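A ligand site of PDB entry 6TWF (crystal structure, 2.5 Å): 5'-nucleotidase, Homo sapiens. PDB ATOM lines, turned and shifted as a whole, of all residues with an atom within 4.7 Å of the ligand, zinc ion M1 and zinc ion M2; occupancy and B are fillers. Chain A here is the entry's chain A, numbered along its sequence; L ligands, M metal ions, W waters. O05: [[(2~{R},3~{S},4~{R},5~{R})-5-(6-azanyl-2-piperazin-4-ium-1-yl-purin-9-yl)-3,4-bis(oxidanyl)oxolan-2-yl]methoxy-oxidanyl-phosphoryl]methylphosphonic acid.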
ATOM      1  N   ASP A  11      -0.097 -25.980 -13.327  1.00  0.00           N
ATOM      2  CA  ASP A  11      -0.662 -25.906 -14.670  1.00  0.00           C
ATOM      3  C   ASP A  11      -0.076 -26.976 -15.632  1.00  0.00           C
ATOM      4  O   ASP A  11       0.182 -26.700 -16.804  1.00  0.00           O
ATOM      5  CB  ASP A  11      -0.512 -24.460 -15.196  1.00  0.00           C
ATOM      6  CG  ASP A  11      -1.226 -23.471 -14.298  1.00  0.00           C
ATOM      7  OD1 ASP A  11      -0.759 -23.255 -13.173  1.00  0.00           O
ATOM      8  OD2 ASP A  11      -2.103 -22.731 -14.804  1.00  0.00           O
ATOM      9  N   HIS A  13      -1.646 -29.510 -16.865  1.00  0.00           N
ATOM     10  CA  HIS A  13      -2.655 -29.586 -17.933  1.00  0.00           C
ATOM     11  C   HIS A  13      -2.529 -30.854 -18.830  1.00  0.00           C
ATOM     12  O   HIS A  13      -2.448 -30.760 -20.055  1.00  0.00           O
ATOM     13  CB  HIS A  13      -2.668 -28.270 -18.749  1.00  0.00           C
ATOM     14  CG  HIS A  13      -3.342 -27.151 -18.017  1.00  0.00           C
ATOM     15  ND1 HIS A  13      -4.640 -27.274 -17.560  1.00  0.00           N
ATOM     16  CD2 HIS A  13      -2.870 -25.938 -17.657  1.00  0.00           C
ATOM     17  CE1 HIS A  13      -4.909 -26.159 -16.923  1.00  0.00           C
ATOM     18  NE2 HIS A  13      -3.895 -25.295 -17.023  1.00  0.00           N
ATOM     19  N   ASP A  60      -4.396 -27.119 -11.508  1.00  0.00           N
ATOM     20  CA  ASP A  60      -4.579 -27.203 -12.941  1.00  0.00           C
ATOM     21  C   ASP A  60      -3.816 -28.372 -13.579  1.00  0.00           C
ATOM     22  O   ASP A  60      -3.180 -28.231 -14.630  1.00  0.00           O
ATOM     23  CB  ASP A  60      -4.285 -25.847 -13.609  1.00  0.00           C
ATOM     24  CG  ASP A  60      -5.442 -24.887 -13.699  1.00  0.00           C
ATOM     25  OD1 ASP A  60      -6.481 -25.125 -13.022  1.00  0.00           O
ATOM     26  OD2 ASP A  60      -5.287 -23.834 -14.361  1.00  0.00           O
ATOM     27  N   ASN A  92      -8.638 -23.921 -10.752  1.00  0.00           N
ATOM     28  CA  ASN A  92      -9.941 -23.763 -11.393  1.00  0.00           C
ATOM     29  C   ASN A  92     -10.289 -24.940 -12.297  1.00  0.00           C
ATOM     30  O   ASN A  92     -11.430 -25.400 -12.243  1.00  0.00           O
ATOM     31  CB  ASN A  92     -10.048 -22.416 -12.162  1.00  0.00           C
ATOM     32  CG  ASN A  92      -8.909 -22.132 -13.111  1.00  0.00           C
ATOM     33  OD1 ASN A  92      -7.774 -21.861 -12.705  1.00  0.00           O
ATOM     34  ND2 ASN A  92      -9.171 -22.163 -14.407  1.00  0.00           N
ATOM     35  N   HIS A  93      -9.323 -25.472 -13.073  1.00  0.00           N
ATOM     36  CA  HIS A  93      -9.623 -26.555 -14.011  1.00  0.00           C
ATOM     37  C   HIS A  93      -9.961 -27.886 -13.329  1.00  0.00           C
ATOM     38  O   HIS A  93     -10.616 -28.714 -13.954  1.00  0.00           O
ATOM     39  CB  HIS A  93      -8.523 -26.702 -15.090  1.00  0.00           C
ATOM     40  CG  HIS A  93      -8.631 -25.608 -16.117  1.00  0.00           C
ATOM     41  ND1 HIS A  93      -9.547 -25.653 -17.134  1.00  0.00           N
ATOM     42  CD2 HIS A  93      -7.948 -24.451 -16.207  1.00  0.00           C
ATOM     43  CE1 HIS A  93      -9.420 -24.514 -17.792  1.00  0.00           C
ATOM     44  NE2 HIS A  93      -8.427 -23.786 -17.310  1.00  0.00           N
ATOM     45  N   LEU A 159     -14.988 -19.052 -14.261  1.00  0.00           N
ATOM     46  CA  LEU A 159     -14.071 -19.774 -15.156  1.00  0.00           C
ATOM     47  C   LEU A 159     -14.392 -21.243 -15.376  1.00  0.00           C
ATOM     48  O   LEU A 159     -14.069 -21.781 -16.436  1.00  0.00           O
ATOM     49  CB  LEU A 159     -12.644 -19.721 -14.587  1.00  0.00           C
ATOM     50  CG  LEU A 159     -12.008 -18.351 -14.322  1.00  0.00           C
ATOM     51  CD1 LEU A 159     -10.601 -18.527 -13.694  1.00  0.00           C
ATOM     52  CD2 LEU A 159     -11.988 -17.506 -15.612  1.00  0.00           C
ATOM     53  N   ASN A 161     -16.968 -24.906 -13.646  1.00  0.00           N
ATOM     54  CA  ASN A 161     -18.303 -25.358 -13.288  1.00  0.00           C
ATOM     55  C   ASN A 161     -18.314 -25.945 -11.864  1.00  0.00           C
ATOM     56  O   ASN A 161     -18.671 -27.104 -11.681  1.00  0.00           O
ATOM     57  CB  ASN A 161     -18.778 -26.376 -14.337  1.00  0.00           C
ATOM     58  CG  ASN A 161     -18.596 -25.879 -15.757  1.00  0.00           C
ATOM     59  OD1 ASN A 161     -19.062 -24.802 -16.119  1.00  0.00           O
ATOM     60  ND2 ASN A 161     -17.867 -26.635 -16.587  1.00  0.00           N
ATOM     61  N   HIS A 195      -3.646 -21.560  -6.274  1.00  0.00           N
ATOM     62  CA  HIS A 195      -3.940 -21.337  -7.657  1.00  0.00           C
ATOM     63  C   HIS A 195      -4.756 -20.074  -7.978  1.00  0.00           C
ATOM     64  O   HIS A 195      -5.950 -20.147  -8.321  1.00  0.00           O
ATOM     65  CB  HIS A 195      -4.641 -22.588  -8.173  1.00  0.00           C
ATOM     66  CG  HIS A 195      -4.637 -22.663  -9.656  1.00  0.00           C
ATOM     67  ND1 HIS A 195      -3.610 -23.267 -10.334  1.00  0.00           N
ATOM     68  CD2 HIS A 195      -5.501 -22.149 -10.551  1.00  0.00           C
ATOM     69  CE1 HIS A 195      -3.873 -23.084 -11.607  1.00  0.00           C
ATOM     70  NE2 HIS A 195      -5.032 -22.493 -11.766  1.00  0.00           N
ATOM     71  N   HIS A 218      -1.548 -20.740 -12.114  1.00  0.00           N
ATOM     72  CA  HIS A 218      -2.625 -20.067 -12.864  1.00  0.00           C
ATOM     73  C   HIS A 218      -2.158 -19.043 -13.929  1.00  0.00           C
ATOM     74  O   HIS A 218      -2.816 -18.924 -14.975  1.00  0.00           O
ATOM     75  CB  HIS A 218      -3.602 -19.398 -11.894  1.00  0.00           C
ATOM     76  CG  HIS A 218      -4.843 -18.851 -12.539  1.00  0.00           C
ATOM     77  ND1 HIS A 218      -5.765 -19.658 -13.108  1.00  0.00           N
ATOM     78  CD2 HIS A 218      -5.257 -17.573 -12.646  1.00  0.00           C
ATOM     79  CE1 HIS A 218      -6.736 -18.873 -13.528  1.00  0.00           C
ATOM     80  NE2 HIS A 218      -6.436 -17.589 -13.324  1.00  0.00           N
ATOM     81  N   ASN A 220       0.895 -19.166 -15.298  1.00  0.00           N
ATOM     82  CA  ASN A 220       1.941 -19.837 -16.083  1.00  0.00           C
ATOM     83  C   ASN A 220       3.238 -19.018 -16.053  1.00  0.00           C
ATOM     84  O   ASN A 220       3.907 -18.875 -17.060  1.00  0.00           O
ATOM     85  CB  ASN A 220       1.474 -20.077 -17.542  1.00  0.00           C
ATOM     86  CG  ASN A 220       0.183 -20.861 -17.676  1.00  0.00           C
ATOM     87  OD1 ASN A 220      -0.203 -21.627 -16.798  1.00  0.00           O
ATOM     88  ND2 ASN A 220      -0.518 -20.744 -18.806  1.00  0.00           N
ATOM     89  N   ARG A 329      -2.084 -14.678 -27.763  1.00  0.00           N
ATOM     90  CA  ARG A 329      -2.553 -13.676 -26.802  1.00  0.00           C
ATOM     91  C   ARG A 329      -1.903 -12.293 -27.076  1.00  0.00           C
ATOM     92  O   ARG A 329      -2.146 -11.371 -26.309  1.00  0.00           O
ATOM     93  CB  ARG A 329      -2.279 -14.116 -25.367  1.00  0.00           C
ATOM     94  CG  ARG A 329      -2.899 -15.479 -25.020  1.00  0.00           C
ATOM     95  CD  ARG A 329      -2.806 -15.717 -23.517  1.00  0.00           C
ATOM     96  NE  ARG A 329      -3.568 -16.723 -22.799  1.00  0.00           N
ATOM     97  CZ  ARG A 329      -3.563 -18.025 -22.962  1.00  0.00           C
ATOM     98  NH1 ARG A 329      -3.009 -18.564 -24.048  1.00  0.00           N
ATOM     99  NH2 ARG A 329      -4.222 -18.799 -22.113  1.00  0.00           N
ATOM    100  N   ASN A 365     -11.324 -15.633 -28.681  1.00  0.00           N
ATOM    101  CA  ASN A 365     -10.385 -15.322 -27.623  1.00  0.00           C
ATOM    102  C   ASN A 365      -9.135 -16.169 -27.793  1.00  0.00           C
ATOM    103  O   ASN A 365      -9.241 -17.396 -27.878  1.00  0.00           O
ATOM    104  CB  ASN A 365     -10.996 -15.546 -26.238  1.00  0.00           C
ATOM    105  CG  ASN A 365     -11.677 -16.885 -26.028  1.00  0.00           C
ATOM    106  OD1 ASN A 365     -12.607 -17.245 -26.734  1.00  0.00           O
ATOM    107  ND2 ASN A 365     -11.228 -17.656 -25.080  1.00  0.00           N
ATOM    108  N   GLY A 367      -6.894 -16.951 -25.737  1.00  0.00           N
ATOM    109  CA  GLY A 367      -6.731 -17.875 -24.612  1.00  0.00           C
ATOM    110  C   GLY A 367      -7.485 -19.197 -24.747  1.00  0.00           C
ATOM    111  O   GLY A 367      -7.217 -20.139 -23.983  1.00  0.00           O
ATOM    112  N   GLY A 368      -8.443 -19.248 -25.682  1.00  0.00           N
ATOM    113  CA  GLY A 368      -9.188 -20.457 -26.010  1.00  0.00           C
ATOM    114  C   GLY A 368      -8.441 -21.412 -26.933  1.00  0.00           C
ATOM    115  O   GLY A 368      -8.941 -22.511 -27.190  1.00  0.00           O
ATOM    116  N   ARG A 370      -5.291 -23.557 -27.147  1.00  0.00           N
ATOM    117  CA  ARG A 370      -4.461 -24.043 -26.060  1.00  0.00           C
ATOM    118  C   ARG A 370      -3.274 -24.945 -26.414  1.00  0.00           C
ATOM    119  O   ARG A 370      -2.578 -25.408 -25.491  1.00  0.00           O
ATOM    120  CB  ARG A 370      -5.391 -24.693 -25.041  1.00  0.00           C
ATOM    121  CG  ARG A 370      -5.988 -23.513 -24.265  1.00  0.00           C
ATOM    122  CD  ARG A 370      -6.893 -23.869 -23.174  1.00  0.00           C
ATOM    123  NE  ARG A 370      -6.142 -24.133 -21.919  1.00  0.00           N
ATOM    124  CZ  ARG A 370      -5.970 -23.284 -20.903  1.00  0.00           C
ATOM    125  NH1 ARG A 370      -5.270 -23.660 -19.842  1.00  0.00           N
ATOM    126  NH2 ARG A 370      -6.514 -22.074 -20.946  1.00  0.00           N
ATOM    127  N   PHE A 392     -11.768 -27.874 -24.300  1.00  0.00           N
ATOM    128  CA  PHE A 392     -12.862 -27.563 -23.384  1.00  0.00           C
ATOM    129  C   PHE A 392     -14.268 -28.003 -23.757  1.00  0.00           C
ATOM    130  O   PHE A 392     -15.157 -27.881 -22.916  1.00  0.00           O
ATOM    131  CB  PHE A 392     -12.909 -26.060 -23.153  1.00  0.00           C
ATOM    132  CG  PHE A 392     -11.639 -25.468 -22.566  1.00  0.00           C
ATOM    133  CD1 PHE A 392     -10.966 -26.105 -21.509  1.00  0.00           C
ATOM    134  CD2 PHE A 392     -11.177 -24.239 -22.981  1.00  0.00           C
ATOM    135  CE1 PHE A 392      -9.793 -25.555 -20.975  1.00  0.00           C
ATOM    136  CE2 PHE A 392     -10.054 -23.665 -22.398  1.00  0.00           C
ATOM    137  CZ  PHE A 392      -9.385 -24.315 -21.388  1.00  0.00           C
ATOM    138  N   GLY A 393     -14.502 -28.470 -24.977  1.00  0.00           N
ATOM    139  CA  GLY A 393     -15.837 -28.890 -25.383  1.00  0.00           C
ATOM    140  C   GLY A 393     -16.833 -27.755 -25.471  1.00  0.00           C
ATOM    141  O   GLY A 393     -18.012 -27.936 -25.158  1.00  0.00           O
ATOM    142  N   GLY A 394     -16.365 -26.583 -25.884  1.00  0.00           N
ATOM    143  CA  GLY A 394     -17.223 -25.420 -26.086  1.00  0.00           C
ATOM    144  C   GLY A 394     -17.905 -25.471 -27.444  1.00  0.00           C
ATOM    145  O   GLY A 394     -17.687 -26.417 -28.198  1.00  0.00           O
ATOM    146  N   PRO A 473     -16.961 -18.092 -29.848  1.00  0.00           N
ATOM    147  CA  PRO A 473     -17.184 -19.132 -28.818  1.00  0.00           C
ATOM    148  C   PRO A 473     -18.311 -18.782 -27.854  1.00  0.00           C
ATOM    149  O   PRO A 473     -18.522 -17.617 -27.551  1.00  0.00           O
ATOM    150  CB  PRO A 473     -15.834 -19.170 -28.090  1.00  0.00           C
ATOM    151  CG  PRO A 473     -14.864 -18.620 -29.056  1.00  0.00           C
ATOM    152  CD  PRO A 473     -15.602 -17.539 -29.735  1.00  0.00           C
ATOM    153  N   ASN A 474     -19.007 -19.797 -27.323  1.00  0.00           N
ATOM    154  CA  ASN A 474     -20.051 -19.585 -26.313  1.00  0.00           C
ATOM    155  C   ASN A 474     -19.484 -18.885 -25.063  1.00  0.00           C
ATOM    156  O   ASN A 474     -20.203 -18.136 -24.418  1.00  0.00           O
ATOM    157  CB  ASN A 474     -20.753 -20.900 -25.929  1.00  0.00           C
ATOM    158  CG  ASN A 474     -19.877 -21.924 -25.198  1.00  0.00           C
ATOM    159  OD1 ASN A 474     -18.676 -22.074 -25.466  1.00  0.00           O
ATOM    160  ND2 ASN A 474     -20.483 -22.712 -24.328  1.00  0.00           N
ATOM    161  N   PHE A 475     -18.178 -19.134 -24.754  1.00  0.00           N
ATOM    162  CA  PHE A 475     -17.459 -18.492 -23.651  1.00  0.00           C
ATOM    163  C   PHE A 475     -17.581 -16.962 -23.751  1.00  0.00           C
ATOM    164  O   PHE A 475     -17.860 -16.314 -22.741  1.00  0.00           O
ATOM    165  CB  PHE A 475     -15.986 -18.940 -23.673  1.00  0.00           C
ATOM    166  CG  PHE A 475     -15.207 -18.539 -22.435  1.00  0.00           C
ATOM    167  CD1 PHE A 475     -15.452 -19.143 -21.214  1.00  0.00           C
ATOM    168  CD2 PHE A 475     -14.268 -17.511 -22.487  1.00  0.00           C
ATOM    169  CE1 PHE A 475     -14.730 -18.782 -20.066  1.00  0.00           C
ATOM    170  CE2 PHE A 475     -13.587 -17.121 -21.347  1.00  0.00           C
ATOM    171  CZ  PHE A 475     -13.809 -17.764 -20.148  1.00  0.00           C
ATOM    172  N   ASP A 481     -14.141 -13.806 -20.165  1.00  0.00           N
ATOM    173  CA  ASP A 481     -12.951 -12.975 -20.425  1.00  0.00           C
ATOM    174  C   ASP A 481     -13.207 -11.460 -20.296  1.00  0.00           C
ATOM    175  O   ASP A 481     -12.470 -10.671 -20.881  1.00  0.00           O
ATOM    176  CB  ASP A 481     -12.297 -13.323 -21.804  1.00  0.00           C
ATOM    177  CG  ASP A 481     -11.163 -14.356 -21.739  1.00  0.00           C
ATOM    178  OD1 ASP A 481     -10.766 -14.753 -20.620  1.00  0.00           O
ATOM    179  OD2 ASP A 481     -10.712 -14.790 -22.818  1.00  0.00           O
HETATM  180  C2  O05 L   1     -14.498 -22.270 -22.182  1.00  0.00           C
HETATM  181  C3  O05 L   1      -6.224 -19.465 -16.946  1.00  0.00           C
HETATM  182  C4  O05 L   1     -12.686 -20.959 -22.013  1.00  0.00           C
HETATM  183  C5  O05 L   1     -12.550 -20.843 -23.376  1.00  0.00           C
HETATM  184  C6  O05 L   1     -13.477 -21.559 -24.173  1.00  0.00           C
HETATM  185  C8  O05 L   1     -11.019 -19.633 -22.543  1.00  0.00           C
HETATM  186  C9  O05 L   1     -15.725 -23.218 -20.241  1.00  0.00           C
HETATM  187  C10 O05 L   1     -15.910 -24.724 -20.213  1.00  0.00           C
HETATM  188  C11 O05 L   1     -16.942 -24.649 -22.401  1.00  0.00           C
HETATM  189  C12 O05 L   1     -16.811 -23.157 -22.412  1.00  0.00           C
HETATM  190  O2A O05 L   1      -4.983 -20.004 -19.495  1.00  0.00           O
HETATM  191  PA  O05 L   1      -5.645 -18.994 -18.578  1.00  0.00           P
HETATM  192  O1A O05 L   1      -4.624 -17.843 -18.310  1.00  0.00           O
HETATM  193  PB  O05 L   1      -5.755 -21.124 -16.487  1.00  0.00           P
HETATM  194  O3B O05 L   1      -4.283 -21.165 -16.258  1.00  0.00           O
HETATM  195  O1B O05 L   1      -6.222 -22.055 -17.625  1.00  0.00           O
HETATM  196  O2B O05 L   1      -6.599 -21.503 -15.260  1.00  0.00           O
HETATM  197  O5' O05 L   1      -7.036 -18.406 -19.038  1.00  0.00           O
HETATM  198  C5' O05 L   1      -8.068 -19.096 -19.807  1.00  0.00           C
HETATM  199  C4' O05 L   1      -9.360 -19.240 -19.022  1.00  0.00           C
HETATM  200  O4' O05 L   1     -10.490 -18.932 -19.876  1.00  0.00           O
HETATM  201  C3' O05 L   1      -9.636 -20.639 -18.476  1.00  0.00           C
HETATM  202  O7  O05 L   1     -10.341 -20.585 -17.246  1.00  0.00           O
HETATM  203  C2' O05 L   1     -10.456 -21.282 -19.595  1.00  0.00           C
HETATM  204  O8  O05 L   1     -11.353 -22.298 -19.163  1.00  0.00           O
HETATM  205  C1' O05 L   1     -11.287 -20.087 -20.066  1.00  0.00           C
HETATM  206  N9  O05 L   1     -11.682 -20.179 -21.474  1.00  0.00           N
HETATM  207  N7  O05 L   1     -11.502 -20.010 -23.713  1.00  0.00           N
HETATM  208  N6  O05 L   1     -13.487 -21.554 -25.501  1.00  0.00           N
HETATM  209  N3  O05 L   1     -13.608 -21.654 -21.347  1.00  0.00           N
HETATM  210  N1  O05 L   1     -14.433 -22.268 -23.542  1.00  0.00           N
HETATM  211  N2  O05 L   1     -15.643 -22.742 -21.615  1.00  0.00           N
HETATM  212  N4  O05 L   1     -17.082 -25.115 -21.011  1.00  0.00           N
HETATM  213 ZN    ZN M   1      -5.878 -21.921 -13.571  1.00  0.00          ZN
HETATM  214 ZN    ZN M   2      -3.699 -23.500 -16.001  1.00  0.00          ZN
HETATM  215  O   HOH W   1      -2.598 -22.908 -17.500  1.00  0.00           O
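OD2 of Asp 11 lies close to OD1 of Asn 220 (3.0 Å). The side-chain carboxylate of Asp 60 lies within hydrogen-bond range of the backbone NH of His 93. The side-chain amide nitrogen (ND2) of Asn 365 sits close to the backbone NH (N) of Gly 368. A ring nitrogen (NE2) of His 93 sits close to the side-chain amide nitrogen (ND2) of Asn 92, at 3.4 Å. The side-chain carboxylate (OD1) of Asp 11 is in hydrogen-bond range of the backbone NH (N) of His 218, 2.8 Å away.
Four residues have an atom within 4 Å of zinc ion M1: Asp 60, Asn 92, His 195 and His 218. The nearest printed residue that does not touch zinc ion M1 is Asp 11 (4.1 Å).
Zinc ion M1 is bound by an oxygen (O2B) of the ligand (1.9 Å), a ring nitrogen (NE2) of His 195 (2.1 Å), the side-chain amide oxygen of Asn 92 (2.1 Å), the side-chain carboxylate of Asp 60 (2.2 Å) and a ring nitrogen (ND1) of His 218 (2.3 Å). Zinc ion M1 has five donor atoms within binding distance.
Zinc ion M2 is bound by water W1, a ring nitrogen (NE2) of His 13, the side-chain carboxylate (OD2) of Asp 11, the side-chain carboxylate (OD2) of Asp 60 and an oxygen (O3B) of the ligand.
Residues that only touch the ligand: Phe 475, Gly 368, Phe 392, Leu 159, Asn 474 and Gly 394. Within 4 Å of the ligand: Asp 11, Asp 60, Asn 92, His 93, Leu 159, His 195, His 218, Arg 329, Asn 365, Gly 368, Arg 370, Phe 392, Gly 394, Asn 474 and Phe 475. The nearest printed residue that does not touch the ligand is His 13 (4.03 Å).
A ring nitrogen (NE2) of His 93 lies within hydrogen-bond range of an oxygen (O1B) of the ligand (2.8 Å). NH1 of Arg 370 lies within salt-bridge range of O1B of the ligand, at 2.9 Å. O2A of the ligand lies within salt-bridge range of NH2 of Arg 329. A nitrogen (N7) of the ligand is in hydrogen-bond range of the side-chain amide nitrogen of Asn 365.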
